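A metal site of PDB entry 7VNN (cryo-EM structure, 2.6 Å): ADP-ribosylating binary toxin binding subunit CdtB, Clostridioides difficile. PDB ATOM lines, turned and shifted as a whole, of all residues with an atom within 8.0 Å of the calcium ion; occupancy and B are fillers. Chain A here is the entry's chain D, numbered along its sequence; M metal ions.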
ATOM      1  N   LEU A 362      -5.180  -5.049 -17.582  1.00  0.00           N
ATOM      2  CA  LEU A 362      -4.668  -5.200 -16.230  1.00  0.00           C
ATOM      3  C   LEU A 362      -3.260  -4.618 -16.149  1.00  0.00           C
ATOM      4  O   LEU A 362      -2.465  -4.740 -17.080  1.00  0.00           O
ATOM      5  CB  LEU A 362      -4.652  -6.666 -15.797  1.00  0.00           C
ATOM      6  CG  LEU A 362      -5.876  -7.500 -16.188  1.00  0.00           C
ATOM      7  CD1 LEU A 362      -5.701  -8.938 -15.722  1.00  0.00           C
ATOM      8  CD2 LEU A 362      -7.144  -6.899 -15.603  1.00  0.00           C
ATOM      9  N   SER A 373      -6.967  -8.479  -8.344  1.00  0.00           N
ATOM     10  CA  SER A 373      -7.142  -9.910  -8.134  1.00  0.00           C
ATOM     11  C   SER A 373      -5.817 -10.662  -8.056  1.00  0.00           C
ATOM     12  O   SER A 373      -5.835 -11.877  -7.802  1.00  0.00           O
ATOM     13  CB  SER A 373      -7.989 -10.504  -9.270  1.00  0.00           C
ATOM     14  OG  SER A 373      -7.294 -10.460 -10.495  1.00  0.00           O
ATOM     15  N   CYS A 374      -4.687  -9.995  -8.240  1.00  0.00           N
ATOM     16  CA  CYS A 374      -3.386 -10.644  -8.236  1.00  0.00           C
ATOM     17  C   CYS A 374      -2.493 -10.195  -7.091  1.00  0.00           C
ATOM     18  O   CYS A 374      -1.379 -10.716  -6.951  1.00  0.00           O
ATOM     19  CB  CYS A 374      -2.672 -10.404  -9.573  1.00  0.00           C
ATOM     20  SG  CYS A 374      -3.714 -10.691 -11.031  1.00  0.00           S
ATOM     21  N   PHE A 418       2.503 -17.015  -7.191  1.00  0.00           N
ATOM     22  CA  PHE A 418       1.191 -16.721  -7.764  1.00  0.00           C
ATOM     23  C   PHE A 418       1.037 -17.509  -9.065  1.00  0.00           C
ATOM     24  O   PHE A 418       2.019 -17.924  -9.673  1.00  0.00           O
ATOM     25  CB  PHE A 418       1.025 -15.216  -8.008  1.00  0.00           C
ATOM     26  CG  PHE A 418      -0.307 -14.841  -8.582  1.00  0.00           C
ATOM     27  CD1 PHE A 418      -1.429 -14.755  -7.779  1.00  0.00           C
ATOM     28  CD2 PHE A 418      -0.441 -14.552  -9.933  1.00  0.00           C
ATOM     29  CE1 PHE A 418      -2.652 -14.404  -8.306  1.00  0.00           C
ATOM     30  CE2 PHE A 418      -1.656 -14.204 -10.465  1.00  0.00           C
ATOM     31  CZ  PHE A 418      -2.770 -14.128  -9.646  1.00  0.00           C
ATOM     32  N   THR A 419      -0.213 -17.718  -9.463  1.00  0.00           N
ATOM     33  CA  THR A 419      -0.507 -18.327 -10.744  1.00  0.00           C
ATOM     34  C   THR A 419      -1.914 -17.929 -11.177  1.00  0.00           C
ATOM     35  O   THR A 419      -2.833 -17.870 -10.346  1.00  0.00           O
ATOM     36  CB  THR A 419      -0.380 -19.863 -10.685  1.00  0.00           C
ATOM     37  OG1 THR A 419      -0.677 -20.421 -11.970  1.00  0.00           O
ATOM     38  CG2 THR A 419      -1.330 -20.456  -9.643  1.00  0.00           C
ATOM     39  N   ASN A 420      -2.070 -17.612 -12.459  1.00  0.00           N
ATOM     40  CA  ASN A 420      -3.371 -17.375 -13.051  1.00  0.00           C
ATOM     41  C   ASN A 420      -3.731 -18.414 -14.097  1.00  0.00           C
ATOM     42  O   ASN A 420      -4.791 -18.318 -14.718  1.00  0.00           O
ATOM     43  CB  ASN A 420      -3.438 -15.980 -13.675  1.00  0.00           C
ATOM     44  CG  ASN A 420      -2.261 -15.690 -14.576  1.00  0.00           C
ATOM     45  OD1 ASN A 420      -1.307 -16.474 -14.640  1.00  0.00           O
ATOM     46  ND2 ASN A 420      -2.317 -14.582 -15.295  1.00  0.00           N
ATOM     47  N   PHE A 421      -2.864 -19.402 -14.309  1.00  0.00           N
ATOM     48  CA  PHE A 421      -3.039 -20.482 -15.277  1.00  0.00           C
ATOM     49  C   PHE A 421      -3.191 -19.995 -16.705  1.00  0.00           C
ATOM     50  O   PHE A 421      -3.651 -20.742 -17.572  1.00  0.00           O
ATOM     51  CB  PHE A 421      -4.237 -21.374 -14.914  1.00  0.00           C
ATOM     52  CG  PHE A 421      -4.321 -21.725 -13.449  1.00  0.00           C
ATOM     53  CD1 PHE A 421      -3.274 -22.371 -12.816  1.00  0.00           C
ATOM     54  CD2 PHE A 421      -5.452 -21.410 -12.721  1.00  0.00           C
ATOM     55  CE1 PHE A 421      -3.349 -22.695 -11.480  1.00  0.00           C
ATOM     56  CE2 PHE A 421      -5.535 -21.732 -11.379  1.00  0.00           C
ATOM     57  CZ  PHE A 421      -4.483 -22.374 -10.759  1.00  0.00           C
ATOM     58  N   ASP A 422      -2.825 -18.746 -16.987  1.00  0.00           N
ATOM     59  CA  ASP A 422      -2.880 -18.195 -18.341  1.00  0.00           C
ATOM     60  C   ASP A 422      -1.493 -17.889 -18.891  1.00  0.00           C
ATOM     61  O   ASP A 422      -1.108 -18.404 -19.941  1.00  0.00           O
ATOM     62  CB  ASP A 422      -3.750 -16.937 -18.361  1.00  0.00           C
ATOM     63  CG  ASP A 422      -5.228 -17.244 -18.417  1.00  0.00           C
ATOM     64  OD1 ASP A 422      -5.612 -18.379 -18.050  1.00  0.00           O
ATOM     65  OD2 ASP A 422      -6.006 -16.353 -18.819  1.00  0.00           O
ATOM     66  N   ASP A 423      -0.738 -17.041 -18.201  1.00  0.00           N
ATOM     67  CA  ASP A 423       0.632 -16.728 -18.609  1.00  0.00           C
ATOM     68  C   ASP A 423       1.622 -16.628 -17.459  1.00  0.00           C
ATOM     69  O   ASP A 423       2.826 -16.581 -17.732  1.00  0.00           O
ATOM     70  CB  ASP A 423       0.656 -15.409 -19.406  1.00  0.00           C
ATOM     71  CG  ASP A 423       0.077 -14.242 -18.640  1.00  0.00           C
ATOM     72  OD1 ASP A 423      -0.425 -14.446 -17.512  1.00  0.00           O
ATOM     73  OD2 ASP A 423       0.120 -13.104 -19.153  1.00  0.00           O
ATOM     74  N   ASP A 440     -13.077 -20.521 -17.821  1.00  0.00           N
ATOM     75  CA  ASP A 440     -13.725 -20.145 -16.569  1.00  0.00           C
ATOM     76  C   ASP A 440     -12.746 -19.390 -15.699  1.00  0.00           C
ATOM     77  O   ASP A 440     -11.621 -19.105 -16.125  1.00  0.00           O
ATOM     78  CB  ASP A 440     -14.272 -21.378 -15.852  1.00  0.00           C
ATOM     79  CG  ASP A 440     -15.269 -22.151 -16.687  1.00  0.00           C
ATOM     80  OD1 ASP A 440     -16.064 -21.518 -17.410  1.00  0.00           O
ATOM     81  OD2 ASP A 440     -15.263 -23.398 -16.634  1.00  0.00           O
ATOM     82  N   GLY A 441     -13.136 -19.053 -14.481  1.00  0.00           N
ATOM     83  CA  GLY A 441     -12.291 -18.244 -13.614  1.00  0.00           C
ATOM     84  C   GLY A 441     -12.333 -16.781 -14.010  1.00  0.00           C
ATOM     85  O   GLY A 441     -12.983 -16.372 -14.981  1.00  0.00           O
ATOM     86  N   LEU A 442     -11.612 -15.970 -13.226  1.00  0.00           N
ATOM     87  CA  LEU A 442     -11.569 -14.537 -13.514  1.00  0.00           C
ATOM     88  C   LEU A 442     -10.874 -14.257 -14.839  1.00  0.00           C
ATOM     89  O   LEU A 442     -11.332 -13.405 -15.616  1.00  0.00           O
ATOM     90  CB  LEU A 442     -10.866 -13.803 -12.370  1.00  0.00           C
ATOM     91  CG  LEU A 442     -11.590 -13.793 -11.018  1.00  0.00           C
ATOM     92  CD1 LEU A 442     -10.733 -13.102  -9.976  1.00  0.00           C
ATOM     93  CD2 LEU A 442     -12.943 -13.118 -11.134  1.00  0.00           C
ATOM     94  N   GLN A 443      -9.771 -14.960 -15.115  1.00  0.00           N
ATOM     95  CA  GLN A 443      -9.061 -14.820 -16.387  1.00  0.00           C
ATOM     96  C   GLN A 443      -8.865 -16.234 -16.952  1.00  0.00           C
ATOM     97  O   GLN A 443      -7.808 -16.847 -16.757  1.00  0.00           O
ATOM     98  CB  GLN A 443      -7.723 -14.099 -16.218  1.00  0.00           C
ATOM     99  CG  GLN A 443      -7.803 -12.595 -15.958  1.00  0.00           C
ATOM    100  CD  GLN A 443      -8.370 -12.238 -14.589  1.00  0.00           C
ATOM    101  OE1 GLN A 443      -9.394 -11.572 -14.480  1.00  0.00           O
ATOM    102  NE2 GLN A 443      -7.692 -12.683 -13.540  1.00  0.00           N
ATOM    103  N   GLY A 444      -9.887 -16.731 -17.654  1.00  0.00           N
ATOM    104  CA  GLY A 444      -9.836 -17.963 -18.417  1.00  0.00           C
ATOM    105  C   GLY A 444      -9.053 -19.126 -17.838  1.00  0.00           C
ATOM    106  O   GLY A 444      -8.120 -19.623 -18.477  1.00  0.00           O
ATOM    107  N   SER A 445      -9.427 -19.588 -16.646  1.00  0.00           N
ATOM    108  CA  SER A 445      -8.669 -20.653 -15.988  1.00  0.00           C
ATOM    109  C   SER A 445      -9.504 -21.283 -14.883  1.00  0.00           C
ATOM    110  O   SER A 445     -10.176 -20.581 -14.127  1.00  0.00           O
ATOM    111  CB  SER A 445      -7.367 -20.106 -15.413  1.00  0.00           C
ATOM    112  OG  SER A 445      -7.603 -18.981 -14.581  1.00  0.00           O
ATOM    113  N   ALA A 446      -9.451 -22.611 -14.804  1.00  0.00           N
ATOM    114  CA  ALA A 446     -10.210 -23.344 -13.792  1.00  0.00           C
ATOM    115  C   ALA A 446      -9.308 -24.147 -12.858  1.00  0.00           C
ATOM    116  O   ALA A 446      -9.395 -23.972 -11.635  1.00  0.00           O
ATOM    117  CB  ALA A 446     -11.208 -24.279 -14.476  1.00  0.00           C
ATOM    118  N   LEU A 532     -11.240 -22.847  -9.563  1.00  0.00           N
ATOM    119  CA  LEU A 532     -10.207 -22.123  -8.845  1.00  0.00           C
ATOM    120  C   LEU A 532      -9.532 -21.139  -9.790  1.00  0.00           C
ATOM    121  O   LEU A 532      -9.499 -21.348 -11.011  1.00  0.00           O
ATOM    122  CB  LEU A 532      -9.167 -23.064  -8.239  1.00  0.00           C
ATOM    123  CG  LEU A 532      -9.639 -24.014  -7.134  1.00  0.00           C
ATOM    124  CD1 LEU A 532      -8.499 -24.910  -6.688  1.00  0.00           C
ATOM    125  CD2 LEU A 532     -10.204 -23.236  -5.963  1.00  0.00           C
ATOM    126  N   ASP A 533      -8.989 -20.072  -9.228  1.00  0.00           N
ATOM    127  CA  ASP A 533      -8.279 -19.093 -10.038  1.00  0.00           C
ATOM    128  C   ASP A 533      -7.482 -18.168  -9.135  1.00  0.00           C
ATOM    129  O   ASP A 533      -7.898 -17.864  -8.004  1.00  0.00           O
ATOM    130  CB  ASP A 533      -9.261 -18.273 -10.896  1.00  0.00           C
ATOM    131  CG  ASP A 533      -8.575 -17.592 -12.064  1.00  0.00           C
ATOM    132  OD1 ASP A 533      -7.341 -17.768 -12.216  1.00  0.00           O
ATOM    133  OD2 ASP A 533      -9.268 -16.902 -12.836  1.00  0.00           O
ATOM    134  N   ASN A 534      -6.323 -17.723  -9.637  1.00  0.00           N
ATOM    135  CA  ASN A 534      -5.480 -16.729  -8.970  1.00  0.00           C
ATOM    136  C   ASN A 534      -5.072 -17.173  -7.570  1.00  0.00           C
ATOM    137  O   ASN A 534      -5.413 -16.553  -6.561  1.00  0.00           O
ATOM    138  CB  ASN A 534      -6.177 -15.359  -8.945  1.00  0.00           C
ATOM    139  CG  ASN A 534      -6.448 -14.820 -10.334  1.00  0.00           C
ATOM    140  OD1 ASN A 534      -5.865 -15.269 -11.318  1.00  0.00           O
ATOM    141  ND2 ASN A 534      -7.345 -13.844 -10.415  1.00  0.00           N
ATOM    142  N   LEU A 535      -4.316 -18.271  -7.517  1.00  0.00           N
ATOM    143  CA  LEU A 535      -3.827 -18.792  -6.247  1.00  0.00           C
ATOM    144  C   LEU A 535      -2.507 -18.128  -5.875  1.00  0.00           C
ATOM    145  O   LEU A 535      -1.561 -18.124  -6.663  1.00  0.00           O
ATOM    146  CB  LEU A 535      -3.640 -20.306  -6.332  1.00  0.00           C
ATOM    147  CG  LEU A 535      -4.845 -21.132  -6.790  1.00  0.00           C
ATOM    148  CD1 LEU A 535      -4.557 -22.617  -6.644  1.00  0.00           C
ATOM    149  CD2 LEU A 535      -6.095 -20.751  -6.025  1.00  0.00           C
HETATM  150 CA    CA M   1      -7.069 -16.676 -14.401  1.00  0.00          CA
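OD1 of Asp 533 sits close to OD1 of Asn 534. The side-chain carboxylate of Asp 533 lies close to the backbone NH of Leu 442. The side-chain amide nitrogen of Asn 534 lies close to the side-chain amide nitrogen of Gln 443 (3.4 Å). The side-chain amide nitrogen (ND2) of Asn 420 is in hydrogen-bond range of the side-chain carboxylate (OD1) of Asp 423, 2.9 Å away. ND2 of Asn 534 lies within hydrogen-bond range of OG of Ser 373.
Residues that only touch the calcium ion: Asn 534 (3.6 Å). Five residues have an atom within 4 Å of the calcium ion: Asn 420, Gln 443, Ser 445, Asp 533 and Asn 534.
The calcium ion is bound by the side-chain hydroxyl (OG) of Ser 445 (2.4 Å), the side-chain carboxylate (OD1) of Asp 533 (2.5 Å), the backbone carbonyl oxygen (O) of Gln 443 (2.5 Å), the side-chain carboxylate (OD2) of Asp 533 (2.7 Å) and the backbone carbonyl oxygen (O) of Asn 420 (2.8 Å).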
